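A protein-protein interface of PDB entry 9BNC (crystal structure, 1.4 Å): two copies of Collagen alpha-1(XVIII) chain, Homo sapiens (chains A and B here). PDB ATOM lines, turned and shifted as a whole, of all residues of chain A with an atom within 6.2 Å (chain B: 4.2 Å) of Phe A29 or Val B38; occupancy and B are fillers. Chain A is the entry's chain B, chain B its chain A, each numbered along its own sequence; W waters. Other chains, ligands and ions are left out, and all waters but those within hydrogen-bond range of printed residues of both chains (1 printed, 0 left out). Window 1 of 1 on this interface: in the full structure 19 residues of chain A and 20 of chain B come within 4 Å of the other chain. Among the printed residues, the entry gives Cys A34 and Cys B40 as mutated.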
ATOM      1  N   VAL A   6     -17.223   2.139  20.203  1.00  0.00           N
ATOM      2  CA  VAL A   6     -16.560   3.230  19.509  1.00  0.00           C
ATOM      3  C   VAL A   6     -17.587   4.307  19.204  1.00  0.00           C
ATOM      4  O   VAL A   6     -18.624   4.001  18.584  1.00  0.00           O
ATOM      5  CB  VAL A   6     -15.927   2.746  18.185  1.00  0.00           C
ATOM      6  CG1 VAL A   6     -15.089   3.835  17.561  1.00  0.00           C
ATOM      7  CG2 VAL A   6     -15.105   1.485  18.359  1.00  0.00           C
ATOM      8  N   ARG A   7     -17.316   5.532  19.607  1.00  0.00           N
ATOM      9  CA  ARG A   7     -18.138   6.701  19.314  1.00  0.00           C
ATOM     10  C   ARG A   7     -17.453   7.514  18.233  1.00  0.00           C
ATOM     11  O   ARG A   7     -16.227   7.565  18.178  1.00  0.00           O
ATOM     12  CB  ARG A   7     -18.316   7.583  20.549  1.00  0.00           C
ATOM     13  CG  ARG A   7     -19.120   6.938  21.644  1.00  0.00           C
ATOM     14  CD  ARG A   7     -20.609   6.816  21.282  1.00  0.00           C
ATOM     15  NE  ARG A   7     -21.241   8.128  21.198  1.00  0.00           N
ATOM     16  CZ  ARG A   7     -21.299   9.015  22.189  1.00  0.00           C
ATOM     17  NH1 ARG A   7     -20.938   8.700  23.425  1.00  0.00           N
ATOM     18  NH2 ARG A   7     -21.742  10.244  21.935  1.00  0.00           N
ATOM     19  N   LEU A   8     -18.235   8.183  17.403  1.00  0.00           N
ATOM     20  CA  LEU A   8     -17.650   8.943  16.313  1.00  0.00           C
ATOM     21  C   LEU A   8     -18.256  10.328  16.148  1.00  0.00           C
ATOM     22  O   LEU A   8     -19.449  10.555  16.395  1.00  0.00           O
ATOM     23  CB  LEU A   8     -17.629   8.207  14.990  1.00  0.00           C
ATOM     24  CG  LEU A   8     -18.980   7.968  14.405  1.00  0.00           C
ATOM     25  CD1 LEU A   8     -19.202   8.985  13.262  1.00  0.00           C
ATOM     26  CD2 LEU A   8     -19.046   6.539  13.901  1.00  0.00           C
ATOM     27  N   TRP A   9     -17.422  11.260  15.703  1.00  0.00           N
ATOM     28  CA  TRP A   9     -17.812  12.603  15.317  1.00  0.00           C
ATOM     29  C   TRP A   9     -17.138  12.962  14.001  1.00  0.00           C
ATOM     30  O   TRP A   9     -16.063  12.486  13.687  1.00  0.00           O
ATOM     31  CB  TRP A   9     -17.377  13.666  16.357  1.00  0.00           C
ATOM     32  CG  TRP A   9     -18.193  13.665  17.581  1.00  0.00           C
ATOM     33  CD1 TRP A   9     -19.261  14.467  17.825  1.00  0.00           C
ATOM     34  CD2 TRP A   9     -18.022  12.849  18.750  1.00  0.00           C
ATOM     35  NE1 TRP A   9     -19.782  14.186  19.059  1.00  0.00           N
ATOM     36  CE2 TRP A   9     -19.031  13.214  19.652  1.00  0.00           C
ATOM     37  CE3 TRP A   9     -17.105  11.853  19.114  1.00  0.00           C
ATOM     38  CZ2 TRP A   9     -19.169  12.621  20.905  1.00  0.00           C
ATOM     39  CZ3 TRP A   9     -17.249  11.258  20.364  1.00  0.00           C
ATOM     40  CH2 TRP A   9     -18.274  11.647  21.242  1.00  0.00           C
ATOM     41  N   ALA A  10     -17.737  13.900  13.264  1.00  0.00           N
ATOM     42  CA  ALA A  10     -17.213  14.284  11.977  1.00  0.00           C
ATOM     43  C   ALA A  10     -15.977  15.167  12.070  1.00  0.00           C
ATOM     44  O   ALA A  10     -15.078  15.081  11.232  1.00  0.00           O
ATOM     45  CB  ALA A  10     -18.291  15.064  11.207  1.00  0.00           C
ATOM     46  N   MET A  15     -16.453  17.060  18.166  1.00  0.00           N
ATOM     47  CA  MET A  15     -16.062  16.156  19.235  1.00  0.00           C
ATOM     48  C   MET A  15     -15.766  16.894  20.540  1.00  0.00           C
ATOM     49  O   MET A  15     -16.227  16.488  21.612  1.00  0.00           O
ATOM     50  CB  MET A  15     -14.810  15.382  18.800  1.00  0.00           C
ATOM     51  CG  MET A  15     -14.326  14.315  19.794  1.00  0.00           C
ATOM     52  SD  MET A  15     -13.093  15.057  20.932  1.00  0.00           S
ATOM     53  CE  MET A  15     -11.702  15.226  19.815  1.00  0.00           C
ATOM     54  N   LEU A  27     -13.720   3.951  22.832  1.00  0.00           N
ATOM     55  CA  LEU A  27     -12.909   4.590  21.815  1.00  0.00           C
ATOM     56  C   LEU A  27     -13.688   5.744  21.187  1.00  0.00           C
ATOM     57  O   LEU A  27     -14.930   5.739  21.132  1.00  0.00           O
ATOM     58  CB  LEU A  27     -12.453   3.610  20.732  1.00  0.00           C
ATOM     59  CG  LEU A  27     -11.220   2.763  21.068  1.00  0.00           C
ATOM     60  CD1 LEU A  27     -11.379   1.979  22.360  1.00  0.00           C
ATOM     61  CD2 LEU A  27     -10.894   1.808  19.922  1.00  0.00           C
ATOM     62  N   ILE A  28     -12.946   6.728  20.687  1.00  0.00           N
ATOM     63  CA  ILE A  28     -13.460   7.957  20.104  1.00  0.00           C
ATOM     64  C   ILE A  28     -12.789   8.149  18.759  1.00  0.00           C
ATOM     65  O   ILE A  28     -11.555   8.244  18.686  1.00  0.00           O
ATOM     66  CB  ILE A  28     -13.156   9.171  20.991  1.00  0.00           C
ATOM     67  CG1 ILE A  28     -13.881   9.077  22.340  1.00  0.00           C
ATOM     68  CG2 ILE A  28     -13.482  10.476  20.266  1.00  0.00           C
ATOM     69  CD1 ILE A  28     -13.087   9.681  23.498  1.00  0.00           C
ATOM     70  N   PHE A  29     -13.585   8.183  17.683  1.00  0.00           N
ATOM     71  CA  PHE A  29     -13.108   8.404  16.322  1.00  0.00           C
ATOM     72  C   PHE A  29     -13.493   9.797  15.872  1.00  0.00           C
ATOM     73  O   PHE A  29     -14.661  10.190  16.008  1.00  0.00           O
ATOM     74  CB  PHE A  29     -13.745   7.388  15.372  1.00  0.00           C
ATOM     75  CG  PHE A  29     -13.338   7.556  13.934  1.00  0.00           C
ATOM     76  CD1 PHE A  29     -12.095   7.142  13.504  1.00  0.00           C
ATOM     77  CD2 PHE A  29     -14.209   8.115  12.989  1.00  0.00           C
ATOM     78  CE1 PHE A  29     -11.700   7.292  12.190  1.00  0.00           C
ATOM     79  CE2 PHE A  29     -13.815   8.253  11.673  1.00  0.00           C
ATOM     80  CZ  PHE A  29     -12.571   7.837  11.279  1.00  0.00           C
ATOM     81  N   VAL A  30     -12.547  10.529  15.326  1.00  0.00           N
ATOM     82  CA  VAL A  30     -12.773  11.855  14.749  1.00  0.00           C
ATOM     83  C   VAL A  30     -12.488  11.754  13.260  1.00  0.00           C
ATOM     84  O   VAL A  30     -11.358  11.468  12.847  1.00  0.00           O
ATOM     85  CB  VAL A  30     -11.896  12.928  15.402  1.00  0.00           C
ATOM     86  CG1 VAL A  30     -12.227  14.297  14.834  1.00  0.00           C
ATOM     87  CG2 VAL A  30     -12.078  12.926  16.909  1.00  0.00           C
ATOM     88  N   ALA A  31     -13.523  11.958  12.438  1.00  0.00           N
ATOM     89  CA  ALA A  31     -13.414  11.650  11.016  1.00  0.00           C
ATOM     90  C   ALA A  31     -12.499  12.590  10.259  1.00  0.00           C
ATOM     91  O   ALA A  31     -11.830  12.155   9.316  1.00  0.00           O
ATOM     92  CB  ALA A  31     -14.804  11.642  10.388  1.00  0.00           C
ATOM     93  N   GLU A  32     -12.437  13.855  10.675  1.00  0.00           N
ATOM     94  CA  GLU A  32     -11.736  14.900   9.933  1.00  0.00           C
ATOM     95  C   GLU A  32     -10.278  14.551   9.706  1.00  0.00           C
ATOM     96  O   GLU A  32      -9.784  14.631   8.575  1.00  0.00           O
ATOM     97  CB  GLU A  32     -11.893  16.191  10.754  1.00  0.00           C
ATOM     98  CG  GLU A  32     -11.195  17.437  10.263  1.00  0.00           C
ATOM     99  CD  GLU A  32     -11.631  18.680  11.047  1.00  0.00           C
ATOM    100  OE1 GLU A  32     -11.740  18.619  12.301  1.00  0.00           O
ATOM    101  OE2 GLU A  32     -11.876  19.721  10.400  1.00  0.00           O
ATOM    102  N   CYS A  34      -9.138  11.434  10.719  1.00  0.00           N
ATOM    103  CA  CYS A  34      -9.129   9.980  10.859  1.00  0.00           C
ATOM    104  C   CYS A  34      -8.287   9.570  12.074  1.00  0.00           C
ATOM    105  O   CYS A  34      -7.314   8.821  11.968  1.00  0.00           O
ATOM    106  CB  CYS A  34      -8.659   9.266   9.583  1.00  0.00           C
ATOM    107  SG  CYS A  34      -9.016   7.473   9.539  1.00  0.00           S
ATOM    108  N   GLU A  35      -8.679  10.074  13.240  1.00  0.00           N
ATOM    109  CA  GLU A  35      -7.947   9.853  14.473  1.00  0.00           C
ATOM    110  C   GLU A  35      -8.774   9.103  15.492  1.00  0.00           C
ATOM    111  O   GLU A  35     -10.008   9.144  15.477  1.00  0.00           O
ATOM    112  CB  GLU A  35      -7.499  11.177  15.088  1.00  0.00           C
ATOM    113  CG  GLU A  35      -6.561  11.905  14.154  1.00  0.00           C
ATOM    114  CD  GLU A  35      -5.895  13.104  14.772  1.00  0.00           C
ATOM    115  OE1 GLU A  35      -6.529  13.768  15.615  1.00  0.00           O
ATOM    116  OE2 GLU A  35      -4.739  13.385  14.388  1.00  0.00           O
ATOM    117  N   LEU A  36      -8.083   8.429  16.395  1.00  0.00           N
ATOM    118  CA  LEU A  36      -8.693   7.622  17.429  1.00  0.00           C
ATOM    119  C   LEU A  36      -8.104   7.959  18.785  1.00  0.00           C
ATOM    120  O   LEU A  36      -6.886   8.143  18.924  1.00  0.00           O
ATOM    121  CB  LEU A  36      -8.460   6.132  17.182  1.00  0.00           C
ATOM    122  CG  LEU A  36      -9.371   5.395  16.218  1.00  0.00           C
ATOM    123  CD1 LEU A  36      -8.765   4.009  15.989  1.00  0.00           C
ATOM    124  CD2 LEU A  36     -10.772   5.306  16.782  1.00  0.00           C
ATOM    125  N   TYR A  37      -8.972   8.020  19.787  1.00  0.00           N
ATOM    126  CA  TYR A  37      -8.603   8.217  21.179  1.00  0.00           C
ATOM    127  C   TYR A  37      -9.291   7.156  22.027  1.00  0.00           C
ATOM    128  O   TYR A  37     -10.301   6.561  21.622  1.00  0.00           O
ATOM    129  CB  TYR A  37      -9.059   9.584  21.706  1.00  0.00           C
ATOM    130  CG  TYR A  37      -8.439  10.749  21.007  1.00  0.00           C
ATOM    131  CD1 TYR A  37      -8.947  11.220  19.785  1.00  0.00           C
ATOM    132  CD2 TYR A  37      -7.315  11.380  21.542  1.00  0.00           C
ATOM    133  CE1 TYR A  37      -8.332  12.285  19.120  1.00  0.00           C
ATOM    134  CE2 TYR A  37      -6.709  12.458  20.890  1.00  0.00           C
ATOM    135  CZ  TYR A  37      -7.221  12.892  19.691  1.00  0.00           C
ATOM    136  OH  TYR A  37      -6.604  13.969  19.053  1.00  0.00           O
ATOM    137  N   LEU A  49      -1.395   5.884  15.025  1.00  0.00           N
ATOM    138  CA  LEU A  49      -1.847   5.379  13.737  1.00  0.00           C
ATOM    139  C   LEU A  49      -0.799   5.676  12.669  1.00  0.00           C
ATOM    140  O   LEU A  49      -0.221   6.765  12.639  1.00  0.00           O
ATOM    141  CB  LEU A  49      -3.159   6.043  13.312  1.00  0.00           C
ATOM    142  CG  LEU A  49      -4.335   5.862  14.243  1.00  0.00           C
ATOM    143  CD1 LEU A  49      -5.562   6.607  13.742  1.00  0.00           C
ATOM    144  CD2 LEU A  49      -4.687   4.420  14.412  1.00  0.00           C
ATOM    145  N   GLY B  25     -15.204   4.971  10.107  1.00  0.00           N
ATOM    146  CA  GLY B  25     -15.087   5.004  11.542  1.00  0.00           C
ATOM    147  C   GLY B  25     -15.092   3.657  12.229  1.00  0.00           C
ATOM    148  O   GLY B  25     -14.949   3.606  13.453  1.00  0.00           O
ATOM    149  N   TRP B  26     -15.274   2.571  11.480  1.00  0.00           N
ATOM    150  CA  TRP B  26     -15.162   1.235  12.033  1.00  0.00           C
ATOM    151  C   TRP B  26     -13.718   0.781  12.028  1.00  0.00           C
ATOM    152  O   TRP B  26     -12.919   1.153  11.163  1.00  0.00           O
ATOM    153  CB  TRP B  26     -16.010   0.267  11.208  1.00  0.00           C
ATOM    154  CG  TRP B  26     -17.500   0.377  11.504  1.00  0.00           C
ATOM    155  CD1 TRP B  26     -18.331   1.416  11.192  1.00  0.00           C
ATOM    156  CD2 TRP B  26     -18.303  -0.582  12.177  1.00  0.00           C
ATOM    157  NE1 TRP B  26     -19.602   1.158  11.645  1.00  0.00           N
ATOM    158  CE2 TRP B  26     -19.608  -0.054  12.262  1.00  0.00           C
ATOM    159  CE3 TRP B  26     -18.036  -1.809  12.758  1.00  0.00           C
ATOM    160  CZ2 TRP B  26     -20.647  -0.741  12.888  1.00  0.00           C
ATOM    161  CZ3 TRP B  26     -19.076  -2.493  13.371  1.00  0.00           C
ATOM    162  CH2 TRP B  26     -20.357  -1.945  13.433  1.00  0.00           C
ATOM    163  N   TYR B  37      -6.834  -1.993  11.806  1.00  0.00           N
ATOM    164  CA  TYR B  37      -6.916  -0.781  11.026  1.00  0.00           C
ATOM    165  C   TYR B  37      -8.174  -0.025  11.397  1.00  0.00           C
ATOM    166  O   TYR B  37      -9.098  -0.578  12.011  1.00  0.00           O
ATOM    167  CB  TYR B  37      -7.021  -1.062   9.513  1.00  0.00           C
ATOM    168  CG  TYR B  37      -5.862  -1.871   8.941  1.00  0.00           C
ATOM    169  CD1 TYR B  37      -5.829  -3.253   9.067  1.00  0.00           C
ATOM    170  CD2 TYR B  37      -4.849  -1.253   8.236  1.00  0.00           C
ATOM    171  CE1 TYR B  37      -4.801  -3.979   8.539  1.00  0.00           C
ATOM    172  CE2 TYR B  37      -3.789  -1.992   7.698  1.00  0.00           C
ATOM    173  CZ  TYR B  37      -3.793  -3.352   7.874  1.00  0.00           C
ATOM    174  OH  TYR B  37      -2.774  -4.131   7.337  1.00  0.00           O
ATOM    175  N   VAL B  38      -8.232   1.238  11.014  1.00  0.00           N
ATOM    176  CA  VAL B  38      -9.466   2.015  11.072  1.00  0.00           C
ATOM    177  C   VAL B  38      -9.801   2.526   9.684  1.00  0.00           C
ATOM    178  O   VAL B  38      -8.919   2.886   8.906  1.00  0.00           O
ATOM    179  CB  VAL B  38      -9.369   3.138  12.116  1.00  0.00           C
ATOM    180  CG1 VAL B  38      -8.354   4.151  11.754  1.00  0.00           C
ATOM    181  CG2 VAL B  38     -10.726   3.804  12.357  1.00  0.00           C
ATOM    182  N   ARG B  39     -11.090   2.521   9.358  1.00  0.00           N
ATOM    183  CA  ARG B  39     -11.544   3.020   8.065  1.00  0.00           C
ATOM    184  C   ARG B  39     -11.801   4.523   8.124  1.00  0.00           C
ATOM    185  O   ARG B  39     -12.587   5.022   8.944  1.00  0.00           O
ATOM    186  CB  ARG B  39     -12.790   2.295   7.555  1.00  0.00           C
ATOM    187  CG  ARG B  39     -13.407   2.850   6.241  1.00  0.00           C
ATOM    188  CD  ARG B  39     -12.671   2.326   4.997  1.00  0.00           C
ATOM    189  NE  ARG B  39     -13.297   2.657   3.704  1.00  0.00           N
ATOM    190  CZ  ARG B  39     -14.126   1.872   3.013  1.00  0.00           C
ATOM    191  NH1 ARG B  39     -14.546   0.701   3.480  1.00  0.00           N
ATOM    192  NH2 ARG B  39     -14.553   2.280   1.822  1.00  0.00           N
ATOM    193  N   CYS B  40     -11.142   5.238   7.229  1.00  0.00           N
ATOM    194  CA  CYS B  40     -11.312   6.678   7.056  1.00  0.00           C
ATOM    195  C   CYS B  40     -12.263   6.958   5.905  1.00  0.00           C
ATOM    196  O   CYS B  40     -12.652   6.066   5.169  1.00  0.00           O
ATOM    197  CB  CYS B  40      -9.987   7.350   6.703  1.00  0.00           C
ATOM    198  SG  CYS B  40      -8.567   6.839   7.657  1.00  0.00           S
ATOM    199  N   PHE B  44      -7.505   4.106   4.768  1.00  0.00           N
ATOM    200  CA  PHE B  44      -7.353   3.266   5.934  1.00  0.00           C
ATOM    201  C   PHE B  44      -6.124   3.725   6.692  1.00  0.00           C
ATOM    202  O   PHE B  44      -5.129   4.131   6.073  1.00  0.00           O
ATOM    203  CB  PHE B  44      -7.159   1.786   5.544  1.00  0.00           C
ATOM    204  CG  PHE B  44      -8.327   1.210   4.797  1.00  0.00           C
ATOM    205  CD1 PHE B  44      -8.475   1.453   3.452  1.00  0.00           C
ATOM    206  CD2 PHE B  44      -9.296   0.446   5.435  1.00  0.00           C
ATOM    207  CE1 PHE B  44      -9.561   0.986   2.755  1.00  0.00           C
ATOM    208  CE2 PHE B  44     -10.363  -0.035   4.709  1.00  0.00           C
ATOM    209  CZ  PHE B  44     -10.505   0.235   3.375  1.00  0.00           C
ATOM    210  N   ARG B  45      -6.137   3.576   8.023  1.00  0.00           N
ATOM    211  CA  ARG B  45      -4.945   3.803   8.845  1.00  0.00           C
ATOM    212  C   ARG B  45      -4.679   2.592   9.711  1.00  0.00           C
ATOM    213  O   ARG B  45      -5.594   2.098  10.380  1.00  0.00           O
ATOM    214  CB  ARG B  45      -5.066   5.055   9.699  1.00  0.00           C
ATOM    215  CG  ARG B  45      -5.168   6.305   8.875  1.00  0.00           C
ATOM    216  CD  ARG B  45      -5.188   7.565   9.718  1.00  0.00           C
ATOM    217  NE  ARG B  45      -3.884   7.846  10.309  1.00  0.00           N
ATOM    218  CZ  ARG B  45      -3.607   8.907  11.041  1.00  0.00           C
ATOM    219  NH1 ARG B  45      -4.547   9.769  11.383  1.00  0.00           N
ATOM    220  NH2 ARG B  45      -2.343   9.134  11.389  1.00  0.00           N
HETATM  221  O   HOH W   1       0.678   8.926  10.820  1.00  0.00           O
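The side-chain sulfur (SG) of Cys A34 is disulfide-bonded to the side-chain sulfur (SG) of Cys B40 (2.0 Å).
The backbone carbonyl oxygen (O) of Cys A34 sits at hydrogen-bond distance from the guanidinium group (NH1) of Arg B45 (3.0 Å).
NH2 of Arg B45 sits at hydrogen-bond distance from O of Leu A49.
The backbone NH of Gly B25 sits at hydrogen-bond distance from the backbone carbonyl oxygen of Arg B39 (2.9 Å).
The backbone carbonyl oxygen (O) of Trp B26 sits at hydrogen-bond distance from the backbone NH (N) of Arg B39.
The backbone NH of Val B38 sits at hydrogen-bond distance from the backbone carbonyl oxygen of Arg B45 (2.8 Å).
The backbone carbonyl oxygen (O) of Arg A7 sits at hydrogen-bond distance from the backbone NH (N) of Phe A29 (2.8 Å).
The backbone NH of Trp A9 sits at hydrogen-bond distance from the backbone carbonyl oxygen of Phe A29 (3.0 Å).
Phe A29 touches Gly B25 (CE2 to CA, 3.5 Å).
Val B38 touches Phe A29 (CG2 to CE1, 3.6 Å).
CZ of Phe A29 touches O of Arg B39, 3.7 Å away.
Of the printed residues of chain B, Phe A29 touches Gly B25 (3.5 Å), Val B38 (3.6 Å) and Arg B39 (3.7 Å).
Val A30 touches none of the printed residues of chain B.
Of the printed residues of chain A, Val B38 touches Phe A29 (3.6 Å).
Of the printed residues of chain A, Arg B39 touches Phe A29 (3.7 Å).
Printed residues of chain A within 4 Å of Cys B40: Cys A34 (2.0 Å).
Printed residues of chain A within 4 Å of Arg B45: Cys A34 (3.0 Å) and Leu A49 (3.4 Å).
The nearest printed residue of chain A that does not touch Val B38 is Leu A36 (4.02 Å).
The nearest printed residue of chain A that does not touch Cys B40 is Phe A29 (4.6 Å).
Of the 8 printed residues of chain B, 5 touch a printed residue of chain A.
Hydrophobic or aromatic side chains of chain B that line the printed part of chain A: Val B38.
Among the printed residues, 6 pairs touch across the chains.
Among the printed residues, no Asp or Glu carboxylate lies within 4 Å of a Lys or Arg side-chain nitrogen of the other chain.
1 position is printed for both chains.
Of the 6 pairs that touch across the chains among the printed residues, none has its exchanged pair printed and touching as well.
Water W1 lies within hydrogen-bond range of O of Leu A49 (3.0 Å) and NH2 of Arg B45 (3.1 Å).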
